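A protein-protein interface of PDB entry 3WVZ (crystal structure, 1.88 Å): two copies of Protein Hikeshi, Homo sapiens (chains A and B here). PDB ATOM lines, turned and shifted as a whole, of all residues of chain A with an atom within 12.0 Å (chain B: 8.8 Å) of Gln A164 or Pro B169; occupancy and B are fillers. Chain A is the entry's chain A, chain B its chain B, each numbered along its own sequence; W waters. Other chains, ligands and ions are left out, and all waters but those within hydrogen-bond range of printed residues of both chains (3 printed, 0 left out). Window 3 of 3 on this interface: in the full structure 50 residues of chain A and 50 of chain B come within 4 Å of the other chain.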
ATOM      1  N   PHE A 160      -0.556  35.250 -26.092  1.00  0.00           N
ATOM      2  CA  PHE A 160      -0.432  35.304 -24.640  1.00  0.00           C
ATOM      3  C   PHE A 160      -0.591  33.934 -23.984  1.00  0.00           C
ATOM      4  O   PHE A 160      -0.642  33.836 -22.753  1.00  0.00           O
ATOM      5  CB  PHE A 160      -1.459  36.281 -24.065  1.00  0.00           C
ATOM      6  CG  PHE A 160      -1.199  37.713 -24.441  1.00  0.00           C
ATOM      7  CD1 PHE A 160      -1.756  38.257 -25.585  1.00  0.00           C
ATOM      8  CD2 PHE A 160      -0.382  38.511 -23.655  1.00  0.00           C
ATOM      9  CE1 PHE A 160      -1.508  39.575 -25.941  1.00  0.00           C
ATOM     10  CE2 PHE A 160      -0.129  39.827 -24.006  1.00  0.00           C
ATOM     11  CZ  PHE A 160      -0.694  40.360 -25.148  1.00  0.00           C
ATOM     12  N   ALA A 161      -0.666  32.884 -24.800  1.00  0.00           N
ATOM     13  CA  ALA A 161      -0.883  31.537 -24.276  1.00  0.00           C
ATOM     14  C   ALA A 161       0.311  31.091 -23.442  1.00  0.00           C
ATOM     15  O   ALA A 161       1.462  31.274 -23.836  1.00  0.00           O
ATOM     16  CB  ALA A 161      -1.138  30.552 -25.402  1.00  0.00           C
ATOM     17  N   VAL A 162       0.020  30.495 -22.296  1.00  0.00           N
ATOM     18  CA  VAL A 162       1.051  30.130 -21.343  1.00  0.00           C
ATOM     19  C   VAL A 162       0.665  28.833 -20.634  1.00  0.00           C
ATOM     20  O   VAL A 162      -0.514  28.585 -20.371  1.00  0.00           O
ATOM     21  CB  VAL A 162       1.262  31.276 -20.320  1.00  0.00           C
ATOM     22  CG1 VAL A 162      -0.046  31.600 -19.603  1.00  0.00           C
ATOM     23  CG2 VAL A 162       2.322  30.938 -19.326  1.00  0.00           C
ATOM     24  N   SER A 163       1.648  27.986 -20.355  1.00  0.00           N
ATOM     25  CA  SER A 163       1.378  26.775 -19.594  1.00  0.00           C
ATOM     26  C   SER A 163       1.431  27.107 -18.112  1.00  0.00           C
ATOM     27  O   SER A 163       1.891  28.179 -17.737  1.00  0.00           O
ATOM     28  CB  SER A 163       2.382  25.674 -19.933  1.00  0.00           C
ATOM     29  OG  SER A 163       3.671  26.007 -19.458  1.00  0.00           O
ATOM     30  N   GLN A 164       0.967  26.189 -17.271  1.00  0.00           N
ATOM     31  CA  GLN A 164       1.026  26.401 -15.827  1.00  0.00           C
ATOM     32  C   GLN A 164       2.460  26.597 -15.346  1.00  0.00           C
ATOM     33  O   GLN A 164       2.720  27.404 -14.452  1.00  0.00           O
ATOM     34  CB  GLN A 164       0.375  25.230 -15.091  1.00  0.00           C
ATOM     35  CG  GLN A 164      -1.124  25.148 -15.314  1.00  0.00           C
ATOM     36  CD  GLN A 164      -1.765  23.996 -14.574  1.00  0.00           C
ATOM     37  OE1 GLN A 164      -1.103  23.279 -13.826  1.00  0.00           O
ATOM     38  NE2 GLN A 164      -3.061  23.809 -14.782  1.00  0.00           N
ATOM     39  N   ALA A 165       3.392  25.876 -15.959  1.00  0.00           N
ATOM     40  CA  ALA A 165       4.798  25.961 -15.580  1.00  0.00           C
ATOM     41  C   ALA A 165       5.424  27.301 -15.963  1.00  0.00           C
ATOM     42  O   ALA A 165       6.430  27.709 -15.384  1.00  0.00           O
ATOM     43  CB  ALA A 165       5.578  24.816 -16.213  1.00  0.00           C
ATOM     44  N   GLN A 166       4.830  27.982 -16.938  1.00  0.00           N
ATOM     45  CA  GLN A 166       5.377  29.243 -17.430  1.00  0.00           C
ATOM     46  C   GLN A 166       4.706  30.458 -16.769  1.00  0.00           C
ATOM     47  O   GLN A 166       5.145  31.592 -16.955  1.00  0.00           O
ATOM     48  CB  GLN A 166       5.229  29.334 -18.955  1.00  0.00           C
ATOM     49  CG  GLN A 166       5.830  28.188 -19.761  1.00  0.00           C
ATOM     50  CD  GLN A 166       5.292  28.119 -21.192  1.00  0.00           C
ATOM     51  OE1 GLN A 166       4.158  28.517 -21.469  1.00  0.00           O
ATOM     52  NE2 GLN A 166       6.111  27.611 -22.108  1.00  0.00           N
ATOM     53  N   MET A 167       3.648  30.215 -16.000  1.00  0.00           N
ATOM     54  CA  MET A 167       2.876  31.297 -15.380  1.00  0.00           C
ATOM     55  C   MET A 167       3.587  32.034 -14.255  1.00  0.00           C
ATOM     56  O   MET A 167       4.388  31.457 -13.524  1.00  0.00           O
ATOM     57  CB  MET A 167       1.561  30.758 -14.819  1.00  0.00           C
ATOM     58  CG  MET A 167       0.518  30.478 -15.853  1.00  0.00           C
ATOM     59  SD  MET A 167      -0.962  29.760 -15.131  1.00  0.00           S
ATOM     60  CE  MET A 167      -1.845  29.360 -16.650  1.00  0.00           C
ATOM     61  N   THR A 168       3.264  33.316 -14.120  1.00  0.00           N
ATOM     62  CA  THR A 168       3.617  34.079 -12.932  1.00  0.00           C
ATOM     63  C   THR A 168       2.393  34.144 -12.018  1.00  0.00           C
ATOM     64  O   THR A 168       1.264  34.238 -12.501  1.00  0.00           O
ATOM     65  CB  THR A 168       4.097  35.503 -13.284  1.00  0.00           C
ATOM     66  OG1 THR A 168       3.031  36.233 -13.903  1.00  0.00           O
ATOM     67  CG2 THR A 168       5.284  35.446 -14.234  1.00  0.00           C
ATOM     68  N   PRO A 169       2.609  34.074 -10.694  1.00  0.00           N
ATOM     69  CA  PRO A 169       1.513  34.123  -9.716  1.00  0.00           C
ATOM     70  C   PRO A 169       0.632  35.364  -9.867  1.00  0.00           C
ATOM     71  O   PRO A 169       1.126  36.487  -9.783  1.00  0.00           O
ATOM     72  CB  PRO A 169       2.245  34.137  -8.372  1.00  0.00           C
ATOM     73  CG  PRO A 169       3.546  33.464  -8.649  1.00  0.00           C
ATOM     74  CD  PRO A 169       3.917  33.871 -10.045  1.00  0.00           C
ATOM     75  N   SER A 170      -0.662  35.154 -10.089  1.00  0.00           N
ATOM     76  CA  SER A 170      -1.605  36.253 -10.267  1.00  0.00           C
ATOM     77  C   SER A 170      -2.997  35.809  -9.823  1.00  0.00           C
ATOM     78  O   SER A 170      -3.837  35.466 -10.653  1.00  0.00           O
ATOM     79  CB  SER A 170      -1.618  36.715 -11.728  1.00  0.00           C
ATOM     80  OG  SER A 170      -2.323  37.935 -11.885  1.00  0.00           O
ATOM     81  N   PRO A 171      -3.243  35.817  -8.501  1.00  0.00           N
ATOM     82  CA  PRO A 171      -4.439  35.222  -7.887  1.00  0.00           C
ATOM     83  C   PRO A 171      -5.760  35.887  -8.278  1.00  0.00           C
ATOM     84  O   PRO A 171      -6.817  35.291  -8.082  1.00  0.00           O
ATOM     85  CB  PRO A 171      -4.180  35.397  -6.386  1.00  0.00           C
ATOM     86  CG  PRO A 171      -3.255  36.560  -6.299  1.00  0.00           C
ATOM     87  CD  PRO A 171      -2.367  36.449  -7.498  1.00  0.00           C
ATOM     88  N   GLU A 173      -6.369  37.029 -11.419  1.00  0.00           N
ATOM     89  CA  GLU A 173      -6.554  36.883 -12.862  1.00  0.00           C
ATOM     90  C   GLU A 173      -7.322  35.612 -13.217  1.00  0.00           C
ATOM     91  O   GLU A 173      -7.186  34.589 -12.545  1.00  0.00           O
ATOM     92  CB  GLU A 173      -5.200  36.878 -13.578  1.00  0.00           C
ATOM     93  CG  GLU A 173      -4.807  38.208 -14.191  1.00  0.00           C
ATOM     94  CD  GLU A 173      -3.602  38.087 -15.105  1.00  0.00           C
ATOM     95  OE1 GLU A 173      -2.662  37.342 -14.758  1.00  0.00           O
ATOM     96  OE2 GLU A 173      -3.604  38.724 -16.179  1.00  0.00           O
ATOM     97  N   MET A 174      -8.126  35.691 -14.276  1.00  0.00           N
ATOM     98  CA  MET A 174      -8.816  34.520 -14.806  1.00  0.00           C
ATOM     99  C   MET A 174      -8.188  34.069 -16.129  1.00  0.00           C
ATOM    100  O   MET A 174      -7.674  34.887 -16.900  1.00  0.00           O
ATOM    101  CB  MET A 174     -10.307  34.814 -15.007  1.00  0.00           C
ATOM    102  CG  MET A 174     -11.031  35.185 -13.718  1.00  0.00           C
ATOM    103  SD  MET A 174     -10.983  33.867 -12.491  1.00  0.00           S
ATOM    104  CE  MET A 174     -12.119  32.692 -13.218  1.00  0.00           C
ATOM    105  N   PHE A 175      -8.233  32.764 -16.373  1.00  0.00           N
ATOM    106  CA  PHE A 175      -7.604  32.164 -17.540  1.00  0.00           C
ATOM    107  C   PHE A 175      -8.586  31.275 -18.286  1.00  0.00           C
ATOM    108  O   PHE A 175      -9.395  30.580 -17.674  1.00  0.00           O
ATOM    109  CB  PHE A 175      -6.379  31.337 -17.138  1.00  0.00           C
ATOM    110  CG  PHE A 175      -5.244  32.157 -16.605  1.00  0.00           C
ATOM    111  CD1 PHE A 175      -5.232  32.566 -15.282  1.00  0.00           C
ATOM    112  CD2 PHE A 175      -4.189  32.516 -17.428  1.00  0.00           C
ATOM    113  CE1 PHE A 175      -4.189  33.326 -14.785  1.00  0.00           C
ATOM    114  CE2 PHE A 175      -3.140  33.275 -16.940  1.00  0.00           C
ATOM    115  CZ  PHE A 175      -3.141  33.678 -15.615  1.00  0.00           C
ATOM    116  N   ILE A 176      -8.503  31.301 -19.611  1.00  0.00           N
ATOM    117  CA  ILE A 176      -9.322  30.430 -20.452  1.00  0.00           C
ATOM    118  C   ILE A 176      -8.436  29.349 -21.071  1.00  0.00           C
ATOM    119  O   ILE A 176      -7.370  29.656 -21.601  1.00  0.00           O
ATOM    120  CB  ILE A 176     -10.034  31.244 -21.562  1.00  0.00           C
ATOM    121  CG1 ILE A 176     -10.745  32.456 -20.950  1.00  0.00           C
ATOM    122  CG2 ILE A 176     -11.011  30.364 -22.342  1.00  0.00           C
ATOM    123  CD1 ILE A 176     -11.210  33.480 -21.956  1.00  0.00           C
ATOM    124  N   PRO A 177      -8.860  28.072 -20.992  1.00  0.00           N
ATOM    125  CA  PRO A 177      -8.064  27.018 -21.636  1.00  0.00           C
ATOM    126  C   PRO A 177      -7.884  27.322 -23.117  1.00  0.00           C
ATOM    127  O   PRO A 177      -8.841  27.739 -23.766  1.00  0.00           O
ATOM    128  CB  PRO A 177      -8.907  25.757 -21.436  1.00  0.00           C
ATOM    129  CG  PRO A 177      -9.770  26.062 -20.252  1.00  0.00           C
ATOM    130  CD  PRO A 177     -10.063  27.534 -20.336  1.00  0.00           C
ATOM    131  N   ALA A 178      -6.674  27.145 -23.633  1.00  0.00           N
ATOM    132  CA  ALA A 178      -6.396  27.463 -25.027  1.00  0.00           C
ATOM    133  C   ALA A 178      -7.272  26.658 -25.998  1.00  0.00           C
ATOM    134  O   ALA A 178      -7.641  27.160 -27.060  1.00  0.00           O
ATOM    135  CB  ALA A 178      -4.922  27.236 -25.332  1.00  0.00           C
ATOM    136  N   ASN A 179      -7.624  25.422 -25.649  1.00  0.00           N
ATOM    137  CA  ASN A 179      -8.414  24.633 -26.588  1.00  0.00           C
ATOM    138  C   ASN A 179      -9.842  25.176 -26.693  1.00  0.00           C
ATOM    139  O   ASN A 179     -10.495  25.003 -27.723  1.00  0.00           O
ATOM    140  CB  ASN A 179      -8.413  23.132 -26.232  1.00  0.00           C
ATOM    141  CG  ASN A 179      -8.951  22.828 -24.838  1.00  0.00           C
ATOM    142  OD1 ASN A 179      -9.356  23.715 -24.092  1.00  0.00           O
ATOM    143  ND2 ASN A 179      -8.956  21.543 -24.486  1.00  0.00           N
ATOM    144  N   VAL B 162     -10.923  29.922 -15.420  1.00  0.00           N
ATOM    145  CA  VAL B 162     -10.467  29.448 -14.117  1.00  0.00           C
ATOM    146  C   VAL B 162      -9.354  30.338 -13.582  1.00  0.00           C
ATOM    147  O   VAL B 162      -8.587  30.924 -14.350  1.00  0.00           O
ATOM    148  CB  VAL B 162      -9.971  27.976 -14.172  1.00  0.00           C
ATOM    149  CG1 VAL B 162     -11.147  27.013 -14.360  1.00  0.00           C
ATOM    150  CG2 VAL B 162      -8.925  27.791 -15.264  1.00  0.00           C
ATOM    151  N   SER B 163      -9.290  30.459 -12.261  1.00  0.00           N
ATOM    152  CA  SER B 163      -8.175  31.137 -11.620  1.00  0.00           C
ATOM    153  C   SER B 163      -7.063  30.119 -11.401  1.00  0.00           C
ATOM    154  O   SER B 163      -7.275  28.921 -11.574  1.00  0.00           O
ATOM    155  CB  SER B 163      -8.600  31.769 -10.291  1.00  0.00           C
ATOM    156  OG  SER B 163      -8.936  30.774  -9.339  1.00  0.00           O
ATOM    157  N   GLN B 164      -5.879  30.592 -11.033  1.00  0.00           N
ATOM    158  CA  GLN B 164      -4.755  29.691 -10.820  1.00  0.00           C
ATOM    159  C   GLN B 164      -5.029  28.737  -9.653  1.00  0.00           C
ATOM    160  O   GLN B 164      -4.590  27.589  -9.664  1.00  0.00           O
ATOM    161  CB  GLN B 164      -3.471  30.490 -10.589  1.00  0.00           C
ATOM    162  CG  GLN B 164      -2.925  31.128 -11.861  1.00  0.00           C
ATOM    163  CD  GLN B 164      -1.809  32.120 -11.598  1.00  0.00           C
ATOM    164  OE1 GLN B 164      -1.606  32.562 -10.468  1.00  0.00           O
ATOM    165  NE2 GLN B 164      -1.079  32.480 -12.649  1.00  0.00           N
ATOM    166  N   ALA B 165      -5.780  29.209  -8.661  1.00  0.00           N
ATOM    167  CA  ALA B 165      -6.136  28.374  -7.516  1.00  0.00           C
ATOM    168  C   ALA B 165      -7.158  27.307  -7.898  1.00  0.00           C
ATOM    169  O   ALA B 165      -7.242  26.258  -7.259  1.00  0.00           O
ATOM    170  CB  ALA B 165      -6.666  29.233  -6.377  1.00  0.00           C
ATOM    171  N   GLN B 166      -7.929  27.577  -8.947  1.00  0.00           N
ATOM    172  CA  GLN B 166      -8.960  26.653  -9.402  1.00  0.00           C
ATOM    173  C   GLN B 166      -8.415  25.649 -10.415  1.00  0.00           C
ATOM    174  O   GLN B 166      -9.098  24.697 -10.787  1.00  0.00           O
ATOM    175  CB  GLN B 166     -10.139  27.424 -10.011  1.00  0.00           C
ATOM    176  CG  GLN B 166     -10.901  28.280  -9.008  1.00  0.00           C
ATOM    177  CD  GLN B 166     -11.722  29.373  -9.669  1.00  0.00           C
ATOM    178  OE1 GLN B 166     -11.785  29.462 -10.897  1.00  0.00           O
ATOM    179  NE2 GLN B 166     -12.351  30.219  -8.855  1.00  0.00           N
ATOM    180  N   MET B 167      -7.179  25.866 -10.859  1.00  0.00           N
ATOM    181  CA  MET B 167      -6.558  24.982 -11.839  1.00  0.00           C
ATOM    182  C   MET B 167      -6.204  23.627 -11.247  1.00  0.00           C
ATOM    183  O   MET B 167      -5.732  23.538 -10.115  1.00  0.00           O
ATOM    184  CB  MET B 167      -5.300  25.622 -12.427  1.00  0.00           C
ATOM    185  CG  MET B 167      -5.584  26.739 -13.401  1.00  0.00           C
ATOM    186  SD  MET B 167      -4.109  27.610 -13.951  1.00  0.00           S
ATOM    187  CE  MET B 167      -4.888  28.921 -14.892  1.00  0.00           C
ATOM    188  N   THR B 168      -6.431  22.576 -12.023  1.00  0.00           N
ATOM    189  CA  THR B 168      -5.991  21.246 -11.636  1.00  0.00           C
ATOM    190  C   THR B 168      -4.610  21.012 -12.236  1.00  0.00           C
ATOM    191  O   THR B 168      -4.306  21.530 -13.310  1.00  0.00           O
ATOM    192  CB  THR B 168      -6.978  20.155 -12.094  1.00  0.00           C
ATOM    193  OG1 THR B 168      -6.992  20.079 -13.525  1.00  0.00           O
ATOM    194  CG2 THR B 168      -8.377  20.464 -11.585  1.00  0.00           C
ATOM    195  N   PRO B 169      -3.758  20.255 -11.524  1.00  0.00           N
ATOM    196  CA  PRO B 169      -2.380  19.991 -11.950  1.00  0.00           C
ATOM    197  C   PRO B 169      -2.269  19.447 -13.373  1.00  0.00           C
ATOM    198  O   PRO B 169      -2.666  18.313 -13.647  1.00  0.00           O
ATOM    199  CB  PRO B 169      -1.899  18.954 -10.933  1.00  0.00           C
ATOM    200  CG  PRO B 169      -2.670  19.281  -9.702  1.00  0.00           C
ATOM    201  CD  PRO B 169      -4.031  19.699 -10.185  1.00  0.00           C
ATOM    202  N   SER B 170      -1.733  20.271 -14.268  1.00  0.00           N
ATOM    203  CA  SER B 170      -1.464  19.869 -15.643  1.00  0.00           C
ATOM    204  C   SER B 170      -0.427  20.802 -16.259  1.00  0.00           C
ATOM    205  O   SER B 170      -0.781  21.698 -17.028  1.00  0.00           O
ATOM    206  CB  SER B 170      -2.750  19.878 -16.473  1.00  0.00           C
ATOM    207  OG  SER B 170      -2.512  19.379 -17.776  1.00  0.00           O
ATOM    208  N   PRO B 171       0.852  20.599 -15.913  1.00  0.00           N
ATOM    209  CA  PRO B 171       1.977  21.445 -16.323  1.00  0.00           C
ATOM    210  C   PRO B 171       2.063  21.738 -17.823  1.00  0.00           C
ATOM    211  O   PRO B 171       2.669  22.741 -18.201  1.00  0.00           O
ATOM    212  CB  PRO B 171       3.190  20.633 -15.866  1.00  0.00           C
ATOM    213  CG  PRO B 171       2.706  19.949 -14.643  1.00  0.00           C
ATOM    214  CD  PRO B 171       1.288  19.553 -14.966  1.00  0.00           C
ATOM    215  N   SER B 172       1.470  20.887 -18.655  1.00  0.00           N
ATOM    216  CA  SER B 172       1.584  21.022 -20.106  1.00  0.00           C
ATOM    217  C   SER B 172       0.463  21.844 -20.761  1.00  0.00           C
ATOM    218  O   SER B 172       0.676  22.457 -21.807  1.00  0.00           O
ATOM    219  CB  SER B 172       1.630  19.637 -20.758  1.00  0.00           C
ATOM    220  OG  SER B 172       0.333  19.204 -21.129  1.00  0.00           O
ATOM    221  N   GLU B 173      -0.722  21.850 -20.157  1.00  0.00           N
ATOM    222  CA  GLU B 173      -1.885  22.494 -20.771  1.00  0.00           C
ATOM    223  C   GLU B 173      -1.700  24.006 -20.908  1.00  0.00           C
ATOM    224  O   GLU B 173      -1.163  24.660 -20.014  1.00  0.00           O
ATOM    225  CB  GLU B 173      -3.153  22.201 -19.966  1.00  0.00           C
ATOM    226  CG  GLU B 173      -4.406  22.157 -20.824  1.00  0.00           C
ATOM    227  CD  GLU B 173      -5.685  22.192 -20.011  1.00  0.00           C
ATOM    228  OE1 GLU B 173      -5.611  22.040 -18.773  1.00  0.00           O
ATOM    229  OE2 GLU B 173      -6.763  22.371 -20.619  1.00  0.00           O
ATOM    230  N   MET B 174      -2.145  24.558 -22.035  1.00  0.00           N
ATOM    231  CA  MET B 174      -1.957  25.984 -22.293  1.00  0.00           C
ATOM    232  C   MET B 174      -3.206  26.775 -21.923  1.00  0.00           C
ATOM    233  O   MET B 174      -4.336  26.320 -22.138  1.00  0.00           O
ATOM    234  CB  MET B 174      -1.599  26.226 -23.765  1.00  0.00           C
ATOM    235  CG  MET B 174      -0.340  25.502 -24.250  1.00  0.00           C
ATOM    236  SD  MET B 174       1.205  26.131 -23.552  1.00  0.00           S
ATOM    237  CE  MET B 174       1.279  27.757 -24.298  1.00  0.00           C
ATOM    238  N   PHE B 175      -2.992  27.966 -21.375  1.00  0.00           N
ATOM    239  CA  PHE B 175      -4.083  28.856 -20.984  1.00  0.00           C
ATOM    240  C   PHE B 175      -3.875  30.252 -21.553  1.00  0.00           C
ATOM    241  O   PHE B 175      -2.744  30.697 -21.730  1.00  0.00           O
ATOM    242  CB  PHE B 175      -4.193  28.954 -19.460  1.00  0.00           C
ATOM    243  CG  PHE B 175      -4.642  27.687 -18.795  1.00  0.00           C
ATOM    244  CD1 PHE B 175      -3.726  26.701 -18.460  1.00  0.00           C
ATOM    245  CD2 PHE B 175      -5.979  27.489 -18.490  1.00  0.00           C
ATOM    246  CE1 PHE B 175      -4.139  25.531 -17.840  1.00  0.00           C
ATOM    247  CE2 PHE B 175      -6.398  26.328 -17.867  1.00  0.00           C
ATOM    248  CZ  PHE B 175      -5.481  25.347 -17.543  1.00  0.00           C
HETATM  249  O   HOH W   1      -5.703  32.159  -8.089  1.00  0.00           O
HETATM  250  O   HOH W   2      -6.046  24.046 -23.370  1.00  0.00           O
HETATM  251  O   HOH W   3      -5.525  33.486 -10.826  1.00  0.00           O
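Water W3 lies within hydrogen-bond range of O of Ser A170, O of Glu A173 and N of Gln B164. Water W1 lies within hydrogen-bond range of N of Ala B165, O of Pro A171 and N of Gln B164. Water W2 lies within hydrogen-bond range of N of Asn A179 (3.1 Å), O of Met B174 (3.1 Å), N of Ala A178 (3.2 Å) and OE2 of Glu B173 (3.3 Å).
Val A162 touches Phe B175, and with the chains exchanged Phe A175 touches Val B162. Gln A164 touches Phe B175, and with the chains exchanged Phe A175 touches Gln B164. Met B167 touches its own counterpart, Met A167. Met A174 touches Gln B166, but with the chains exchanged Gln A166 does not touch Met B174 (4.1 Å).
Ser A163 touches just these residues of chain B: Pro B171, Glu B173 and Met B174. Printed residues of chain B within 4 Å of Gln A164: Met B167 (3.7 Å), Thr B168 (3.0 Å), Pro B169 (3.995 Å), Ser B170 (3.1 Å), Pro B171 (3.9 Å), Glu B173 (3.8 Å) and Phe B175 (3.7 Å). Gln A166 touches none of the printed residues of chain B. Met A167 touches just these residues of chain B: Gln B164 (3.7 Å), Met B167 (3.5 Å) and Phe B175 (3.7 Å). Printed residues of chain B within 4 Å of Phe A175: Val B162, Gln B164, Met B167 and Phe B175. Printed residues of chain B within 4 Å of Pro A177: Met B174 and Phe B175. Of the printed residues of chain A, Gln B164 touches Met A167, Thr A168, Pro A169, Ser A170 and Phe A175. Printed residues of chain A within 4 Å of Pro B169: Gln A164. Met B174 touches just these residues of chain A: Ala A161 (3.6 Å), Val A162 (3.5 Å), Ser A163 (3.7 Å), Pro A177 (3.8 Å) and Ala A178 (2.9 Å).
CA of Ser A163 touches O of Glu B173 (3.3 Å). NE2 of Gln A164 touches CB of Met B167, 3.7 Å away. Pro B169 touches Gln A164. Gln A164 touches Pro B171 (OE1 to N, 3.9 Å). Phe B175 touches Met A167 (CB to CE, 3.7 Å). Glu A173 touches Ser B163 (O to CA, 3.7 Å). CE of Met A174 touches N of Ser B163, 3.7 Å away. Gln B166 touches Met A174. Phe A175 touches Met B167 (CB to CE, 3.6 Å). CB of Phe A175 touches CB of Phe B175 (3.98 Å).
The side-chain hydroxyl (OG) of Ser A170 sits at hydrogen-bond distance from the side-chain carboxylate (OE1) of Glu A173, at 3.0 Å. The backbone NH (N) of Ser B163 lies within hydrogen-bond range of the side-chain amide oxygen (OE1) of Gln B166 (3.0 Å). The side-chain amide oxygen (OE1) of Gln A166 lies within hydrogen-bond range of the backbone NH (N) of Ser A163 (2.8 Å).
The backbone NH (N) of Ser A163 lies within hydrogen-bond range of the side-chain sulfur (SD) of Met B174. N of Phe A175 lies within hydrogen-bond range of O of Val B162, at 2.8 Å. O of Val A162 is in hydrogen-bond range of N of Phe B175, at 2.7 Å. O of Met B174 lies within hydrogen-bond range of N of Ala A178. The backbone carbonyl oxygen (O) of Thr A168 is in hydrogen-bond range of the side-chain amide nitrogen (NE2) of Gln B164, 2.9 Å away. The side-chain amide nitrogen of Gln A164 lies within hydrogen-bond range of the backbone carbonyl oxygen of Thr B168, 3.0 Å away. NE2 of Gln B164 is in hydrogen-bond range of SD of Met A167, at 3.7 Å. The backbone NH (N) of Ser B170 lies within hydrogen-bond range of the side-chain amide oxygen (OE1) of Gln A164, 3.1 Å away. N of Ser A170 lies within hydrogen-bond range of OE1 of Gln B164 (2.8 Å).
Of the 19 printed residues of chain A, 16 touch a printed residue of chain B. Printed residues of chain A that touch a printed residue of chain B: Phe A160, Ala A161, Val A162, Ser A163, Gln A164, Ala A165, Met A167, Thr A168, Pro A169, Ser A170, Glu A173, Met A174, Phe A175, Ile A176, Pro A177 and Ala A178. Hydrophobic or aromatic side chains of chain A that line the printed part of chain B: Ala A161, Val A162, Met A167, Met A174, Phe A175 and Ala A178. Hydrophobic or aromatic side chains of chain B within 4 Å of the printed part of chain A: Val B162, Met B167, Met B174 and Phe B175. Among the printed residues, 35 pairs touch across the chains. Among the printed residues, no Asp or Glu carboxylate lies within 4 Å of a Lys or Arg side-chain nitrogen of the other chain.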
